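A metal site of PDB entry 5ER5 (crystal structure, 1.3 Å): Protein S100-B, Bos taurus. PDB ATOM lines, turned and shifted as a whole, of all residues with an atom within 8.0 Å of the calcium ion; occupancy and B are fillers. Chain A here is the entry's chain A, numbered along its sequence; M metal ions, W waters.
The calcium ion is bound by water W1 (2.3 Å), the backbone carbonyl oxygen (O) of Ser 19 (2.4 Å), the backbone carbonyl oxygen (O) of Asp 24 (2.4 Å), the side-chain carboxylate (OE1) of Glu 32 (2.4 Å), the backbone carbonyl oxygen (O) of Lys 27 (2.4 Å), the backbone carbonyl oxygen (O) of Glu 22 (2.4 Å) and the side-chain carboxylate (OE2) of Glu 32 (2.5 Å).
Water W1 lies within hydrogen-bond range of OE1 of Glu 68 and N of Lys 29.
Of the 20 residues printed, 5 come within 4 Å of the calcium ion. Along chain A the residues within 4 Å of the calcium ion span positions 19 to 32.
The side-chain hydroxyl of Ser 19 sits at hydrogen-bond distance from the backbone carbonyl oxygen of Lys 25. The side-chain hydroxyl (OG) of Ser 19 lies within hydrogen-bond range of the backbone carbonyl oxygen (O) of Phe 15. The side-chain carboxylate (OD2) of Asp 24 lies within salt-bridge range of the side-chain amino group (NZ) of Lys 27 (3.9 Å). The side-chain carboxylate of Asp 24 sits at hydrogen-bond distance from the backbone NH of His 26 (2.8 Å). N of Lys 29 sits close to OE1 of Glu 32, 2.9 Å away. The side-chain carboxylate (OE1) of Glu 22 is in salt-bridge range of the side-chain amino group (NZ) of Lys 29 (3.6 Å).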
ATOM      1  N   PHE A  15     -12.701  17.760  -0.604  1.00  0.00           N
ATOM      2  CA  PHE A  15     -12.575  18.943   0.224  1.00  0.00           C
ATOM      3  C   PHE A  15     -13.362  20.090  -0.368  1.00  0.00           C
ATOM      4  O   PHE A  15     -14.145  20.731   0.317  1.00  0.00           O
ATOM      5  CB  PHE A  15     -11.112  19.334   0.409  1.00  0.00           C
ATOM      6  CG  PHE A  15     -10.936  20.576   1.213  1.00  0.00           C
ATOM      7  CD1 PHE A  15     -10.962  20.526   2.588  1.00  0.00           C
ATOM      8  CD2 PHE A  15     -10.753  21.792   0.591  1.00  0.00           C
ATOM      9  CE1 PHE A  15     -10.795  21.663   3.338  1.00  0.00           C
ATOM     10  CE2 PHE A  15     -10.602  22.944   1.342  1.00  0.00           C
ATOM     11  CZ  PHE A  15     -10.622  22.874   2.724  1.00  0.00           C
ATOM     12  N   HIS A  16     -13.183  20.337  -1.661  1.00  0.00           N
ATOM     13  CA  HIS A  16     -13.858  21.472  -2.279  1.00  0.00           C
ATOM     14  C   HIS A  16     -15.362  21.275  -2.400  1.00  0.00           C
ATOM     15  O   HIS A  16     -16.111  22.256  -2.312  1.00  0.00           O
ATOM     16  CB  HIS A  16     -13.236  21.768  -3.621  1.00  0.00           C
ATOM     17  CG  HIS A  16     -11.948  22.521  -3.482  1.00  0.00           C
ATOM     18  ND1 HIS A  16     -11.912  23.863  -3.191  1.00  0.00           N
ATOM     19  CD2 HIS A  16     -10.673  22.085  -3.483  1.00  0.00           C
ATOM     20  CE1 HIS A  16     -10.647  24.239  -3.080  1.00  0.00           C
ATOM     21  NE2 HIS A  16      -9.881  23.182  -3.242  1.00  0.00           N
ATOM     22  N   TYR A  18     -17.246  20.220  -0.258  1.00  0.00           N
ATOM     23  CA  TYR A  18     -17.799  20.621   1.025  1.00  0.00           C
ATOM     24  C   TYR A  18     -17.374  22.025   1.438  1.00  0.00           C
ATOM     25  O   TYR A  18     -18.221  22.793   1.913  1.00  0.00           O
ATOM     26  CB  TYR A  18     -17.477  19.557   2.104  1.00  0.00           C
ATOM     27  CG  TYR A  18     -18.331  18.345   1.834  1.00  0.00           C
ATOM     28  CD1 TYR A  18     -17.933  17.357   0.943  1.00  0.00           C
ATOM     29  CD2 TYR A  18     -19.585  18.226   2.398  1.00  0.00           C
ATOM     30  CE1 TYR A  18     -18.754  16.297   0.621  1.00  0.00           C
ATOM     31  CE2 TYR A  18     -20.408  17.183   2.082  1.00  0.00           C
ATOM     32  CZ  TYR A  18     -20.002  16.220   1.212  1.00  0.00           C
ATOM     33  OH  TYR A  18     -20.864  15.190   0.926  1.00  0.00           O
ATOM     34  N   SER A  19     -16.122  22.421   1.207  1.00  0.00           N
ATOM     35  CA  SER A  19     -15.673  23.740   1.625  1.00  0.00           C
ATOM     36  C   SER A  19     -16.371  24.831   0.824  1.00  0.00           C
ATOM     37  O   SER A  19     -16.607  25.915   1.350  1.00  0.00           O
ATOM     38  CB  SER A  19     -14.157  23.870   1.500  1.00  0.00           C
ATOM     39  OG  SER A  19     -13.730  23.882   0.151  1.00  0.00           O
ATOM     40  N   GLY A  20     -16.687  24.553  -0.442  1.00  0.00           N
ATOM     41  CA  GLY A  20     -17.245  25.528  -1.348  1.00  0.00           C
ATOM     42  C   GLY A  20     -18.742  25.701  -1.270  1.00  0.00           C
ATOM     43  O   GLY A  20     -19.318  26.344  -2.153  1.00  0.00           O
ATOM     44  N   ARG A  21     -19.389  25.166  -0.226  1.00  0.00           N
ATOM     45  CA  ARG A  21     -20.837  25.287  -0.086  1.00  0.00           C
ATOM     46  C   ARG A  21     -21.218  26.655   0.470  1.00  0.00           C
ATOM     47  O   ARG A  21     -22.094  27.328  -0.095  1.00  0.00           O
ATOM     48  CB  ARG A  21     -21.357  24.182   0.822  1.00  0.00           C
ATOM     49  CG  ARG A  21     -21.217  22.826   0.204  1.00  0.00           C
ATOM     50  CD  ARG A  21     -21.614  21.738   1.168  1.00  0.00           C
ATOM     51  NE  ARG A  21     -21.733  20.479   0.467  1.00  0.00           N
ATOM     52  CZ  ARG A  21     -22.492  19.474   0.872  1.00  0.00           C
ATOM     53  NH1 ARG A  21     -23.188  19.582   2.002  1.00  0.00           N
ATOM     54  NH2 ARG A  21     -22.573  18.377   0.151  1.00  0.00           N
ATOM     55  N   GLU A  22     -20.585  27.078   1.559  1.00  0.00           N
ATOM     56  CA  GLU A  22     -21.017  28.258   2.275  1.00  0.00           C
ATOM     57  C   GLU A  22     -19.829  29.039   2.801  1.00  0.00           C
ATOM     58  O   GLU A  22     -18.751  28.495   3.062  1.00  0.00           O
ATOM     59  CB  GLU A  22     -21.847  27.911   3.503  1.00  0.00           C
ATOM     60  CG  GLU A  22     -23.144  27.246   3.217  1.00  0.00           C
ATOM     61  CD  GLU A  22     -23.891  26.982   4.503  1.00  0.00           C
ATOM     62  OE1 GLU A  22     -23.790  27.812   5.449  1.00  0.00           O
ATOM     63  OE2 GLU A  22     -24.559  25.947   4.592  1.00  0.00           O
ATOM     64  N   GLY A  23     -20.071  30.339   2.992  1.00  0.00           N
ATOM     65  CA  GLY A  23     -19.109  31.184   3.667  1.00  0.00           C
ATOM     66  C   GLY A  23     -17.785  31.192   2.935  1.00  0.00           C
ATOM     67  O   GLY A  23     -17.741  31.335   1.707  1.00  0.00           O
ATOM     68  N   ASP A  24     -16.711  31.043   3.688  1.00  0.00           N
ATOM     69  CA  ASP A  24     -15.389  30.947   3.093  1.00  0.00           C
ATOM     70  C   ASP A  24     -15.339  29.689   2.232  1.00  0.00           C
ATOM     71  O   ASP A  24     -15.547  28.580   2.734  1.00  0.00           O
ATOM     72  CB  ASP A  24     -14.351  30.878   4.217  1.00  0.00           C
ATOM     73  CG  ASP A  24     -12.916  30.891   3.725  1.00  0.00           C
ATOM     74  OD1 ASP A  24     -12.623  30.397   2.620  1.00  0.00           O
ATOM     75  OD2 ASP A  24     -12.056  31.425   4.452  1.00  0.00           O
ATOM     76  N   LYS A  25     -15.153  29.855   0.927  1.00  0.00           N
ATOM     77  CA  LYS A  25     -15.212  28.707   0.023  1.00  0.00           C
ATOM     78  C   LYS A  25     -13.950  27.866   0.080  1.00  0.00           C
ATOM     79  O   LYS A  25     -13.912  26.797  -0.550  1.00  0.00           O
ATOM     80  CB  LYS A  25     -15.499  29.168  -1.415  1.00  0.00           C
ATOM     81  CG  LYS A  25     -16.798  29.976  -1.588  1.00  0.00           C
ATOM     82  CD  LYS A  25     -18.045  29.198  -1.165  1.00  0.00           C
ATOM     83  CE  LYS A  25     -19.311  30.067  -1.235  1.00  0.00           C
ATOM     84  NZ  LYS A  25     -19.841  30.302  -2.603  1.00  0.00           N
ATOM     85  N   HIS A  26     -12.944  28.294   0.850  1.00  0.00           N
ATOM     86  CA  HIS A  26     -11.682  27.587   0.965  1.00  0.00           C
ATOM     87  C   HIS A  26     -11.521  26.830   2.267  1.00  0.00           C
ATOM     88  O   HIS A  26     -10.478  26.199   2.479  1.00  0.00           O
ATOM     89  CB  HIS A  26     -10.521  28.591   0.865  1.00  0.00           C
ATOM     90  CG  HIS A  26     -10.684  29.599  -0.220  1.00  0.00           C
ATOM     91  ND1 HIS A  26     -10.371  29.341  -1.532  1.00  0.00           N
ATOM     92  CD2 HIS A  26     -11.113  30.887  -0.190  1.00  0.00           C
ATOM     93  CE1 HIS A  26     -10.608  30.411  -2.263  1.00  0.00           C
ATOM     94  NE2 HIS A  26     -11.064  31.357  -1.470  1.00  0.00           N
ATOM     95  N   LYS A  27     -12.523  26.864   3.148  1.00  0.00           N
ATOM     96  CA  LYS A  27     -12.463  26.185   4.432  1.00  0.00           C
ATOM     97  C   LYS A  27     -13.804  25.539   4.739  1.00  0.00           C
ATOM     98  O   LYS A  27     -14.852  25.952   4.230  1.00  0.00           O
ATOM     99  CB  LYS A  27     -12.116  27.160   5.573  1.00  0.00           C
ATOM    100  CG  LYS A  27     -10.817  27.917   5.389  1.00  0.00           C
ATOM    101  CD  LYS A  27     -10.530  28.807   6.587  1.00  0.00           C
ATOM    102  CE  LYS A  27      -9.367  29.768   6.366  1.00  0.00           C
ATOM    103  NZ  LYS A  27      -9.427  30.889   7.347  1.00  0.00           N
ATOM    104  N   LEU A  28     -13.750  24.513   5.602  1.00  0.00           N
ATOM    105  CA  LEU A  28     -14.937  23.814   6.088  1.00  0.00           C
ATOM    106  C   LEU A  28     -15.378  24.432   7.417  1.00  0.00           C
ATOM    107  O   LEU A  28     -14.623  24.402   8.400  1.00  0.00           O
ATOM    108  CB  LEU A  28     -14.607  22.348   6.349  1.00  0.00           C
ATOM    109  CG  LEU A  28     -14.142  21.505   5.180  1.00  0.00           C
ATOM    110  CD1 LEU A  28     -13.468  20.245   5.698  1.00  0.00           C
ATOM    111  CD2 LEU A  28     -15.279  21.168   4.275  1.00  0.00           C
ATOM    112  N   LYS A  29     -16.586  24.984   7.430  1.00  0.00           N
ATOM    113  CA  LYS A  29     -17.239  25.312   8.686  1.00  0.00           C
ATOM    114  C   LYS A  29     -17.906  24.059   9.272  1.00  0.00           C
ATOM    115  O   LYS A  29     -17.935  22.991   8.645  1.00  0.00           O
ATOM    116  CB  LYS A  29     -18.253  26.454   8.489  1.00  0.00           C
ATOM    117  CG  LYS A  29     -19.412  26.120   7.584  1.00  0.00           C
ATOM    118  CD  LYS A  29     -20.551  27.144   7.635  1.00  0.00           C
ATOM    119  CE  LYS A  29     -20.107  28.576   7.486  1.00  0.00           C
ATOM    120  NZ  LYS A  29     -21.325  29.434   7.522  1.00  0.00           N
ATOM    121  N   LYS A  30     -18.444  24.184  10.487  1.00  0.00           N
ATOM    122  CA  LYS A  30     -18.957  23.017  11.189  1.00  0.00           C
ATOM    123  C   LYS A  30     -19.977  22.237  10.358  1.00  0.00           C
ATOM    124  O   LYS A  30     -19.913  21.007  10.283  1.00  0.00           O
ATOM    125  CB  LYS A  30     -19.563  23.411  12.522  1.00  0.00           C
ATOM    126  CG  LYS A  30     -18.570  23.753  13.582  1.00  0.00           C
ATOM    127  CD  LYS A  30     -19.284  24.309  14.818  1.00  0.00           C
ATOM    128  CE  LYS A  30     -18.328  24.596  15.932  1.00  0.00           C
ATOM    129  NZ  LYS A  30     -19.017  25.157  17.110  1.00  0.00           N
ATOM    130  N   SER A  31     -20.949  22.932   9.765  1.00  0.00           N
ATOM    131  CA  SER A  31     -21.987  22.208   9.033  1.00  0.00           C
ATOM    132  C   SER A  31     -21.423  21.500   7.819  1.00  0.00           C
ATOM    133  O   SER A  31     -21.861  20.393   7.487  1.00  0.00           O
ATOM    134  CB  SER A  31     -23.112  23.161   8.646  1.00  0.00           C
ATOM    135  OG  SER A  31     -22.631  24.165   7.778  1.00  0.00           O
ATOM    136  N   GLU A  32     -20.434  22.100   7.148  1.00  0.00           N
ATOM    137  CA  GLU A  32     -19.809  21.447   5.996  1.00  0.00           C
ATOM    138  C   GLU A  32     -19.035  20.208   6.425  1.00  0.00           C
ATOM    139  O   GLU A  32     -19.072  19.169   5.748  1.00  0.00           O
ATOM    140  CB  GLU A  32     -18.879  22.441   5.304  1.00  0.00           C
ATOM    141  CG  GLU A  32     -19.622  23.595   4.642  1.00  0.00           C
ATOM    142  CD  GLU A  32     -18.706  24.729   4.197  1.00  0.00           C
ATOM    143  OE1 GLU A  32     -17.596  24.857   4.737  1.00  0.00           O
ATOM    144  OE2 GLU A  32     -19.095  25.498   3.296  1.00  0.00           O
ATOM    145  N   LEU A  33     -18.325  20.306   7.536  1.00  0.00           N
ATOM    146  CA  LEU A  33     -17.570  19.171   8.064  1.00  0.00           C
ATOM    147  C   LEU A  33     -18.490  18.029   8.477  1.00  0.00           C
ATOM    148  O   LEU A  33     -18.198  16.862   8.208  1.00  0.00           O
ATOM    149  CB  LEU A  33     -16.738  19.645   9.246  1.00  0.00           C
ATOM    150  CG  LEU A  33     -15.914  18.592   9.973  1.00  0.00           C
ATOM    151  CD1 LEU A  33     -14.893  17.958   9.066  1.00  0.00           C
ATOM    152  CD2 LEU A  33     -15.237  19.215  11.159  1.00  0.00           C
ATOM    153  N   GLU A  68     -12.472  27.015  11.687  1.00  0.00           N
ATOM    154  CA  GLU A  68     -12.784  26.259  10.484  1.00  0.00           C
ATOM    155  C   GLU A  68     -11.645  25.303  10.186  1.00  0.00           C
ATOM    156  O   GLU A  68     -10.558  25.405  10.755  1.00  0.00           O
ATOM    157  CB  GLU A  68     -13.053  27.195   9.298  1.00  0.00           C
ATOM    158  CG  GLU A  68     -14.192  28.179   9.566  1.00  0.00           C
ATOM    159  CD  GLU A  68     -14.986  28.586   8.338  1.00  0.00           C
ATOM    160  OE1 GLU A  68     -14.931  27.902   7.305  1.00  0.00           O
ATOM    161  OE2 GLU A  68     -15.717  29.595   8.437  1.00  0.00           O
ATOM    162  N   CYS A  69     -11.914  24.356   9.294  1.00  0.00           N
ATOM    163  CA  CYS A  69     -10.914  23.381   8.874  1.00  0.00           C
ATOM    164  C   CYS A  69     -10.419  23.751   7.482  1.00  0.00           C
ATOM    165  O   CYS A  69     -11.172  23.641   6.508  1.00  0.00           O
ATOM    166  CB  CYS A  69     -11.529  21.981   8.880  1.00  0.00           C
ATOM    167  SG  CYS A  69     -10.370  20.676   8.459  1.00  0.00           S
HETATM  168 CA    CA M   1     -16.996  26.855   3.501  1.00  0.00          CA
HETATM  169  O   HOH W   1     -16.964  27.905   5.598  1.00  0.00           O
